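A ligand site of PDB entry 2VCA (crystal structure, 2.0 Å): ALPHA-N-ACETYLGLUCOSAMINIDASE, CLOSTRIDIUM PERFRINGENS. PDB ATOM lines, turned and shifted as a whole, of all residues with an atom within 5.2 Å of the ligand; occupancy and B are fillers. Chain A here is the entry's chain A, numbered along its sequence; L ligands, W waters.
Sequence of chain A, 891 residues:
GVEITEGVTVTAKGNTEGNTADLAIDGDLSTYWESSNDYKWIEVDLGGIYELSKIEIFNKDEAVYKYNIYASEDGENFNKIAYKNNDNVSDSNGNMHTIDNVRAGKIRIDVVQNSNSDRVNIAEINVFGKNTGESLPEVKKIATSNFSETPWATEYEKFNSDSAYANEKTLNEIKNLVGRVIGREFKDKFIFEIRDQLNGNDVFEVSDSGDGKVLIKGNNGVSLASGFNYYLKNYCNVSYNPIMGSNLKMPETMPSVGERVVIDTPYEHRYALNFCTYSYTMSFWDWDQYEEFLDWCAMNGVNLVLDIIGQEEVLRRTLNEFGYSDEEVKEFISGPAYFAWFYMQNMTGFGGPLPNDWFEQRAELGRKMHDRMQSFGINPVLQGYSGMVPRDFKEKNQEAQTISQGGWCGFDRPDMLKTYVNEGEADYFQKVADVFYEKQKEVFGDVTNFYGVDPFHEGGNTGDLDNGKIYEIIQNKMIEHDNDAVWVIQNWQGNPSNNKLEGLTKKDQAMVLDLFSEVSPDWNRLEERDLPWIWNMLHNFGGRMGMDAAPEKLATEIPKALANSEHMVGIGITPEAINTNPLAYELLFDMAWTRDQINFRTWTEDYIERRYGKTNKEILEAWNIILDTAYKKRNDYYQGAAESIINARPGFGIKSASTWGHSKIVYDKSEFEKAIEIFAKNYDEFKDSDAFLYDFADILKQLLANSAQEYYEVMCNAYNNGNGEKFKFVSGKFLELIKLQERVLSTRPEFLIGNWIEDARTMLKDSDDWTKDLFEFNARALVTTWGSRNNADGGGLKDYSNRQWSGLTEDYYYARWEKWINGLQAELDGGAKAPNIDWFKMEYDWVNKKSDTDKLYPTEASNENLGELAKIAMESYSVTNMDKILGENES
An oxygen (O3) of the ligand sits at hydrogen-bond distance from a ring nitrogen (NE2) of His 457 (2.5 Å).
An oxygen (O1) of the ligand sits at hydrogen-bond distance from the side-chain hydroxyl (OH) of Tyr 800 (2.6 Å).
An oxygen (O6) of the ligand lies within hydrogen-bond range of the side-chain hydroxyl (OH) of Tyr 280, at 2.6 Å.
OE2 of Glu 576 sits at hydrogen-bond distance from O1 of the ligand, 2.7 Å away.
NE1 of Trp 341 lies within hydrogen-bond range of O2 of the ligand (2.7 Å).
An oxygen (O5) of the ligand is in hydrogen-bond range of the side-chain amide nitrogen of Asn 274 (3.1 Å).
SG of Cys 276 sits at hydrogen-bond distance from O2 of the ligand (3.3 Å).
Merely in contact with the ligand: Met 344 (3.6 Å), Glu 458 (3.8 Å), Trp 492 (3.5 Å), Leu 515 (3.5 Å), Leu 538 (3.9 Å), Phe 541 (3.7 Å) and Leu 797 (3.6 Å).
The nearest printed residue that does not touch the ligand is Trp 786 (4.2 Å).
The side-chain sulfur of Met 344 lies within hydrogen-bond range of a ring nitrogen (NE2) of His 457 (3.4 Å).
OH of Tyr 280 is in hydrogen-bond range of NE1 of Trp 786 (3.0 Å).
The backbone NH (N) of Asn 346 is in hydrogen-bond range of the backbone carbonyl oxygen (O) of Trp 341 (2.8 Å).
N of Cys 276 sits at hydrogen-bond distance from OD1 of Asn 274 (3.0 Å).
ND2 of Asn 274 is in hydrogen-bond range of O of Thr 574 (2.9 Å).
The side-chain hydroxyl (OG1) of Thr 574 is in hydrogen-bond range of the backbone carbonyl oxygen (O) of Leu 515 (2.7 Å).
The side-chain amide nitrogen (NE2) of Gln 490 lies within hydrogen-bond range of the side-chain sulfur (SD) of Met 344 (3.6 Å).
OE1 of Glu 458 sits at hydrogen-bond distance from NE1 of Trp 408, 2.9 Å away.
Water W2 lies within hydrogen-bond range of the side-chain amide nitrogen (ND2) of Asn 346 (2.7 Å), the side-chain carboxylate (OE1) of Glu 458 (2.8 Å), an oxygen (O2) of the ligand (2.8 Å) and a ring nitrogen (NE2) of His 457 (3.3 Å).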
ATOM      1  N   ASN A 274      11.373  -6.757  20.428  1.00  0.00           N
ATOM      2  CA  ASN A 274      10.128  -7.066  21.120  1.00  0.00           C
ATOM      3  C   ASN A 274      10.479  -8.086  22.202  1.00  0.00           C
ATOM      4  O   ASN A 274      11.458  -8.820  22.055  1.00  0.00           O
ATOM      5  CB  ASN A 274       9.169  -7.715  20.106  1.00  0.00           C
ATOM      6  CG  ASN A 274       7.712  -7.692  20.532  1.00  0.00           C
ATOM      7  OD1 ASN A 274       7.338  -8.205  21.577  1.00  0.00           O
ATOM      8  ND2 ASN A 274       6.875  -7.131  19.677  1.00  0.00           N
ATOM      9  N   CYS A 276       8.854 -10.625  22.446  1.00  0.00           N
ATOM     10  CA  CYS A 276       8.649 -11.797  21.605  1.00  0.00           C
ATOM     11  C   CYS A 276       9.895 -12.249  20.845  1.00  0.00           C
ATOM     12  O   CYS A 276      10.062 -13.440  20.586  1.00  0.00           O
ATOM     13  CB  CYS A 276       7.492 -11.580  20.632  1.00  0.00           C
ATOM     14  SG  CYS A 276       5.887 -11.361  21.416  1.00  0.00           S
ATOM     15  N   TYR A 280      10.646 -16.158  19.768  1.00  0.00           N
ATOM     16  CA  TYR A 280      10.498 -16.622  18.367  1.00  0.00           C
ATOM     17  C   TYR A 280      11.835 -16.729  17.595  1.00  0.00           C
ATOM     18  O   TYR A 280      11.933 -17.532  16.659  1.00  0.00           O
ATOM     19  CB  TYR A 280       9.489 -15.767  17.587  1.00  0.00           C
ATOM     20  CG  TYR A 280       8.055 -15.868  18.090  1.00  0.00           C
ATOM     21  CD1 TYR A 280       7.447 -17.109  18.293  1.00  0.00           C
ATOM     22  CD2 TYR A 280       7.316 -14.723  18.353  1.00  0.00           C
ATOM     23  CE1 TYR A 280       6.143 -17.199  18.759  1.00  0.00           C
ATOM     24  CE2 TYR A 280       6.007 -14.792  18.812  1.00  0.00           C
ATOM     25  CZ  TYR A 280       5.427 -16.035  19.016  1.00  0.00           C
ATOM     26  OH  TYR A 280       4.138 -16.106  19.483  1.00  0.00           O
ATOM     27  N   TRP A 341       6.522 -14.296  27.124  1.00  0.00           N
ATOM     28  CA  TRP A 341       5.201 -14.257  27.740  1.00  0.00           C
ATOM     29  C   TRP A 341       5.247 -14.500  29.239  1.00  0.00           C
ATOM     30  O   TRP A 341       4.316 -14.131  29.948  1.00  0.00           O
ATOM     31  CB  TRP A 341       4.263 -15.215  27.005  1.00  0.00           C
ATOM     32  CG  TRP A 341       4.298 -14.909  25.547  1.00  0.00           C
ATOM     33  CD1 TRP A 341       3.591 -13.930  24.909  1.00  0.00           C
ATOM     34  CD2 TRP A 341       5.144 -15.507  24.568  1.00  0.00           C
ATOM     35  NE1 TRP A 341       3.932 -13.901  23.579  1.00  0.00           N
ATOM     36  CE2 TRP A 341       4.883 -14.862  23.343  1.00  0.00           C
ATOM     37  CE3 TRP A 341       6.091 -16.553  24.600  1.00  0.00           C
ATOM     38  CZ2 TRP A 341       5.522 -15.219  22.154  1.00  0.00           C
ATOM     39  CZ3 TRP A 341       6.731 -16.900  23.411  1.00  0.00           C
ATOM     40  CH2 TRP A 341       6.450 -16.234  22.206  1.00  0.00           C
ATOM     41  N   MET A 344       6.134 -10.845  30.247  1.00  0.00           N
ATOM     42  CA  MET A 344       4.952  -9.988  30.033  1.00  0.00           C
ATOM     43  C   MET A 344       3.743 -10.403  30.874  1.00  0.00           C
ATOM     44  O   MET A 344       2.641  -9.884  30.679  1.00  0.00           O
ATOM     45  CB  MET A 344       4.611  -9.874  28.548  1.00  0.00           C
ATOM     46  CG  MET A 344       5.644  -9.046  27.784  1.00  0.00           C
ATOM     47  SD  MET A 344       5.164  -8.726  26.091  1.00  0.00           S
ATOM     48  CE  MET A 344       5.188 -10.369  25.365  1.00  0.00           C
ATOM     49  N   ASN A 346       1.974 -13.193  31.186  1.00  0.00           N
ATOM     50  CA  ASN A 346       0.919 -13.911  30.471  1.00  0.00           C
ATOM     51  C   ASN A 346       0.825 -15.405  30.805  1.00  0.00           C
ATOM     52  O   ASN A 346      -0.244 -16.002  30.658  1.00  0.00           O
ATOM     53  CB  ASN A 346       1.100 -13.756  28.960  1.00  0.00           C
ATOM     54  CG  ASN A 346       0.932 -12.320  28.494  1.00  0.00           C
ATOM     55  OD1 ASN A 346       0.017 -11.616  28.932  1.00  0.00           O
ATOM     56  ND2 ASN A 346       1.792 -11.887  27.582  1.00  0.00           N
ATOM     57  N   TRP A 408      -4.706 -16.221  30.010  1.00  0.00           N
ATOM     58  CA  TRP A 408      -4.231 -15.711  28.736  1.00  0.00           C
ATOM     59  C   TRP A 408      -3.981 -16.917  27.843  1.00  0.00           C
ATOM     60  O   TRP A 408      -3.136 -17.750  28.149  1.00  0.00           O
ATOM     61  CB  TRP A 408      -2.940 -14.891  28.917  1.00  0.00           C
ATOM     62  CG  TRP A 408      -2.336 -14.381  27.635  1.00  0.00           C
ATOM     63  CD1 TRP A 408      -2.616 -13.204  27.004  1.00  0.00           C
ATOM     64  CD2 TRP A 408      -1.323 -15.025  26.840  1.00  0.00           C
ATOM     65  NE1 TRP A 408      -1.856 -13.080  25.856  1.00  0.00           N
ATOM     66  CE2 TRP A 408      -1.048 -14.173  25.739  1.00  0.00           C
ATOM     67  CE3 TRP A 408      -0.626 -16.234  26.950  1.00  0.00           C
ATOM     68  CZ2 TRP A 408      -0.102 -14.497  24.749  1.00  0.00           C
ATOM     69  CZ3 TRP A 408       0.313 -16.558  25.966  1.00  0.00           C
ATOM     70  CH2 TRP A 408       0.560 -15.694  24.879  1.00  0.00           C
ATOM     71  N   HIS A 457      -0.783  -6.535  30.294  1.00  0.00           N
ATOM     72  CA  HIS A 457      -0.449  -6.735  28.897  1.00  0.00           C
ATOM     73  C   HIS A 457      -1.347  -7.829  28.332  1.00  0.00           C
ATOM     74  O   HIS A 457      -1.284  -8.976  28.783  1.00  0.00           O
ATOM     75  CB  HIS A 457       1.030  -7.085  28.707  1.00  0.00           C
ATOM     76  CG  HIS A 457       1.426  -7.229  27.271  1.00  0.00           C
ATOM     77  ND1 HIS A 457       1.721  -6.143  26.472  1.00  0.00           N
ATOM     78  CD2 HIS A 457       1.566  -8.318  26.488  1.00  0.00           C
ATOM     79  CE1 HIS A 457       2.030  -6.565  25.254  1.00  0.00           C
ATOM     80  NE2 HIS A 457       1.944  -7.872  25.244  1.00  0.00           N
ATOM     81  N   GLU A 458      -2.173  -7.467  27.353  1.00  0.00           N
ATOM     82  CA  GLU A 458      -3.147  -8.364  26.738  1.00  0.00           C
ATOM     83  C   GLU A 458      -4.125  -9.000  27.741  1.00  0.00           C
ATOM     84  O   GLU A 458      -4.514 -10.161  27.600  1.00  0.00           O
ATOM     85  CB  GLU A 458      -2.460  -9.412  25.852  1.00  0.00           C
ATOM     86  CG  GLU A 458      -1.753  -8.812  24.646  1.00  0.00           C
ATOM     87  CD  GLU A 458      -1.440  -9.849  23.575  1.00  0.00           C
ATOM     88  OE1 GLU A 458      -1.190 -11.018  23.921  1.00  0.00           O
ATOM     89  OE2 GLU A 458      -1.454  -9.474  22.384  1.00  0.00           O
ATOM     90  N   GLN A 490       5.302  -0.311  26.632  1.00  0.00           N
ATOM     91  CA  GLN A 490       4.766  -0.696  25.322  1.00  0.00           C
ATOM     92  C   GLN A 490       3.380  -0.105  25.109  1.00  0.00           C
ATOM     93  O   GLN A 490       2.543  -0.158  26.006  1.00  0.00           O
ATOM     94  CB  GLN A 490       4.654  -2.220  25.194  1.00  0.00           C
ATOM     95  CG  GLN A 490       5.952  -2.984  25.322  1.00  0.00           C
ATOM     96  CD  GLN A 490       5.741  -4.458  25.113  1.00  0.00           C
ATOM     97  OE1 GLN A 490       5.484  -4.899  23.991  1.00  0.00           O
ATOM     98  NE2 GLN A 490       5.842  -5.239  26.188  1.00  0.00           N
ATOM     99  N   TRP A 492       0.320  -0.965  23.010  1.00  0.00           N
ATOM    100  CA  TRP A 492      -0.213  -2.052  22.206  1.00  0.00           C
ATOM    101  C   TRP A 492      -1.739  -2.098  22.296  1.00  0.00           C
ATOM    102  O   TRP A 492      -2.296  -2.196  23.382  1.00  0.00           O
ATOM    103  CB  TRP A 492       0.435  -3.383  22.595  1.00  0.00           C
ATOM    104  CG  TRP A 492      -0.128  -4.611  21.901  1.00  0.00           C
ATOM    105  CD1 TRP A 492      -0.726  -5.690  22.502  1.00  0.00           C
ATOM    106  CD2 TRP A 492      -0.127  -4.895  20.488  1.00  0.00           C
ATOM    107  NE1 TRP A 492      -1.099  -6.616  21.552  1.00  0.00           N
ATOM    108  CE2 TRP A 492      -0.749  -6.158  20.307  1.00  0.00           C
ATOM    109  CE3 TRP A 492       0.343  -4.198  19.358  1.00  0.00           C
ATOM    110  CZ2 TRP A 492      -0.920  -6.743  19.052  1.00  0.00           C
ATOM    111  CZ3 TRP A 492       0.166  -4.782  18.095  1.00  0.00           C
ATOM    112  CH2 TRP A 492      -0.458  -6.046  17.957  1.00  0.00           C
ATOM    113  N   LEU A 515       4.172   0.577  19.278  1.00  0.00           N
ATOM    114  CA  LEU A 515       4.667  -0.716  18.819  1.00  0.00           C
ATOM    115  C   LEU A 515       4.502  -0.987  17.328  1.00  0.00           C
ATOM    116  O   LEU A 515       5.316  -1.700  16.736  1.00  0.00           O
ATOM    117  CB  LEU A 515       3.986  -1.833  19.629  1.00  0.00           C
ATOM    118  CG  LEU A 515       4.894  -2.878  20.267  1.00  0.00           C
ATOM    119  CD1 LEU A 515       5.814  -2.246  21.329  1.00  0.00           C
ATOM    120  CD2 LEU A 515       4.058  -3.989  20.879  1.00  0.00           C
ATOM    121  N   LEU A 538       6.903  -2.743  13.518  1.00  0.00           N
ATOM    122  CA  LEU A 538       6.726  -4.085  14.091  1.00  0.00           C
ATOM    123  C   LEU A 538       6.994  -5.138  13.017  1.00  0.00           C
ATOM    124  O   LEU A 538       7.873  -5.991  13.183  1.00  0.00           O
ATOM    125  CB  LEU A 538       5.318  -4.249  14.686  1.00  0.00           C
ATOM    126  CG  LEU A 538       5.108  -5.238  15.851  1.00  0.00           C
ATOM    127  CD1 LEU A 538       3.792  -4.961  16.606  1.00  0.00           C
ATOM    128  CD2 LEU A 538       5.156  -6.708  15.391  1.00  0.00           C
ATOM    129  N   PHE A 541       5.179 -10.882  12.701  1.00  0.00           N
ATOM    130  CA  PHE A 541       4.376 -11.541  13.718  1.00  0.00           C
ATOM    131  C   PHE A 541       4.691 -13.051  13.757  1.00  0.00           C
ATOM    132  O   PHE A 541       4.582 -13.725  12.737  1.00  0.00           O
ATOM    133  CB  PHE A 541       2.885 -11.332  13.445  1.00  0.00           C
ATOM    134  CG  PHE A 541       2.379  -9.956  13.813  1.00  0.00           C
ATOM    135  CD1 PHE A 541       1.665  -9.753  14.989  1.00  0.00           C
ATOM    136  CD2 PHE A 541       2.626  -8.866  12.991  1.00  0.00           C
ATOM    137  CE1 PHE A 541       1.201  -8.490  15.335  1.00  0.00           C
ATOM    138  CE2 PHE A 541       2.156  -7.593  13.330  1.00  0.00           C
ATOM    139  CZ  PHE A 541       1.440  -7.410  14.506  1.00  0.00           C
ATOM    140  N   THR A 574      10.283  -3.409  16.505  1.00  0.00           N
ATOM    141  CA  THR A 574       9.631  -4.231  17.519  1.00  0.00           C
ATOM    142  C   THR A 574       9.152  -5.588  16.953  1.00  0.00           C
ATOM    143  O   THR A 574       8.046  -6.032  17.288  1.00  0.00           O
ATOM    144  CB  THR A 574       8.434  -3.489  18.137  1.00  0.00           C
ATOM    145  OG1 THR A 574       7.658  -2.899  17.094  1.00  0.00           O
ATOM    146  CG2 THR A 574       8.907  -2.370  19.081  1.00  0.00           C
ATOM    147  N   GLU A 576       8.377  -9.478  16.243  1.00  0.00           N
ATOM    148  CA  GLU A 576       8.208 -10.655  17.095  1.00  0.00           C
ATOM    149  C   GLU A 576       9.285 -11.684  16.779  1.00  0.00           C
ATOM    150  O   GLU A 576       9.634 -12.489  17.637  1.00  0.00           O
ATOM    151  CB  GLU A 576       6.807 -11.227  16.956  1.00  0.00           C
ATOM    152  CG  GLU A 576       5.782 -10.297  17.556  1.00  0.00           C
ATOM    153  CD  GLU A 576       4.367 -10.810  17.502  1.00  0.00           C
ATOM    154  OE1 GLU A 576       4.101 -11.976  17.125  1.00  0.00           O
ATOM    155  OE2 GLU A 576       3.500  -9.998  17.838  1.00  0.00           O
ATOM    156  N   GLN A 639      -1.783  -8.288  10.341  1.00  0.00           N
ATOM    157  CA  GLN A 639      -0.716  -8.688  11.244  1.00  0.00           C
ATOM    158  C   GLN A 639       0.270  -9.623  10.542  1.00  0.00           C
ATOM    159  O   GLN A 639       0.071 -10.840  10.493  1.00  0.00           O
ATOM    160  CB  GLN A 639      -1.275  -9.351  12.512  1.00  0.00           C
ATOM    161  CG  GLN A 639      -2.049  -8.406  13.428  1.00  0.00           C
ATOM    162  CD  GLN A 639      -2.316  -9.004  14.801  1.00  0.00           C
ATOM    163  OE1 GLN A 639      -2.154 -10.204  15.009  1.00  0.00           O
ATOM    164  NE2 GLN A 639      -2.730  -8.167  15.745  1.00  0.00           N
ATOM    165  N   TRP A 786       2.261 -24.467  19.902  1.00  0.00           N
ATOM    166  CA  TRP A 786       2.579 -23.355  20.811  1.00  0.00           C
ATOM    167  C   TRP A 786       2.553 -23.822  22.275  1.00  0.00           C
ATOM    168  O   TRP A 786       3.585 -23.883  22.941  1.00  0.00           O
ATOM    169  CB  TRP A 786       1.646 -22.155  20.563  1.00  0.00           C
ATOM    170  CG  TRP A 786       2.258 -20.802  20.816  1.00  0.00           C
ATOM    171  CD1 TRP A 786       2.665 -19.893  19.885  1.00  0.00           C
ATOM    172  CD2 TRP A 786       2.507 -20.194  22.096  1.00  0.00           C
ATOM    173  NE1 TRP A 786       3.153 -18.758  20.489  1.00  0.00           N
ATOM    174  CE2 TRP A 786       3.077 -18.918  21.850  1.00  0.00           C
ATOM    175  CE3 TRP A 786       2.320 -20.606  23.426  1.00  0.00           C
ATOM    176  CZ2 TRP A 786       3.442 -18.043  22.884  1.00  0.00           C
ATOM    177  CZ3 TRP A 786       2.693 -19.731  24.454  1.00  0.00           C
ATOM    178  CH2 TRP A 786       3.249 -18.474  24.179  1.00  0.00           C
ATOM    179  N   LEU A 797      -3.884 -20.405  19.886  1.00  0.00           N
ATOM    180  CA  LEU A 797      -2.467 -20.276  19.510  1.00  0.00           C
ATOM    181  C   LEU A 797      -1.927 -21.281  18.491  1.00  0.00           C
ATOM    182  O   LEU A 797      -0.757 -21.223  18.117  1.00  0.00           O
ATOM    183  CB  LEU A 797      -1.574 -20.267  20.759  1.00  0.00           C
ATOM    184  CG  LEU A 797      -1.618 -19.048  21.682  1.00  0.00           C
ATOM    185  CD1 LEU A 797      -0.893 -19.349  22.990  1.00  0.00           C
ATOM    186  CD2 LEU A 797      -1.039 -17.796  21.019  1.00  0.00           C
ATOM    187  N   TYR A 800       0.437 -20.441  15.434  1.00  0.00           N
ATOM    188  CA  TYR A 800       0.659 -18.995  15.509  1.00  0.00           C
ATOM    189  C   TYR A 800       2.038 -18.648  14.929  1.00  0.00           C
ATOM    190  O   TYR A 800       2.201 -17.644  14.230  1.00  0.00           O
ATOM    191  CB  TYR A 800       0.522 -18.440  16.949  1.00  0.00           C
ATOM    192  CG  TYR A 800       0.736 -16.932  16.981  1.00  0.00           C
ATOM    193  CD1 TYR A 800      -0.333 -16.055  16.829  1.00  0.00           C
ATOM    194  CD2 TYR A 800       2.023 -16.400  17.073  1.00  0.00           C
ATOM    195  CE1 TYR A 800      -0.119 -14.667  16.824  1.00  0.00           C
ATOM    196  CE2 TYR A 800       2.249 -15.043  17.055  1.00  0.00           C
ATOM    197  CZ  TYR A 800       1.178 -14.176  16.930  1.00  0.00           C
ATOM    198  OH  TYR A 800       1.418 -12.830  16.912  1.00  0.00           O
HETATM  199  C1  LIG L   1       1.092 -10.432  19.802  1.00  0.00           C
HETATM  200  C2  LIG L   1       1.951 -11.347  20.660  1.00  0.00           C
HETATM  201  C3  LIG L   1       2.187 -10.698  22.011  1.00  0.00           C
HETATM  202  C4  LIG L   1       2.797  -9.308  21.861  1.00  0.00           C
HETATM  203  C5  LIG L   1       2.045  -8.478  20.829  1.00  0.00           C
HETATM  204  C6  LIG L   1       2.670  -7.163  20.374  1.00  0.00           C
HETATM  205  C7  LIG L   1       1.965 -13.732  20.503  1.00  0.00           C
HETATM  206  C8  LIG L   1       1.199 -15.001  20.698  1.00  0.00           C
HETATM  207  N1  LIG L   1       1.320 -12.645  20.797  1.00  0.00           N
HETATM  208  O1  LIG L   1       1.032 -10.814  18.491  1.00  0.00           O
HETATM  209  O2  LIG L   1       2.957 -11.495  22.824  1.00  0.00           O
HETATM  210  O3  LIG L   1       2.795  -8.608  23.039  1.00  0.00           O
HETATM  211  O4  LIG L   1       1.557  -9.143  19.736  1.00  0.00           O
HETATM  212  O5  LIG L   1       3.830  -7.319  19.678  1.00  0.00           O
HETATM  213  O6  LIG L   1       3.072 -13.769  20.097  1.00  0.00           O
HETATM  214  O   HOH W   1       5.149  -7.279  22.835  1.00  0.00           O
HETATM  215  O   HOH W   2       1.318 -11.101  25.082  1.00  0.00           O
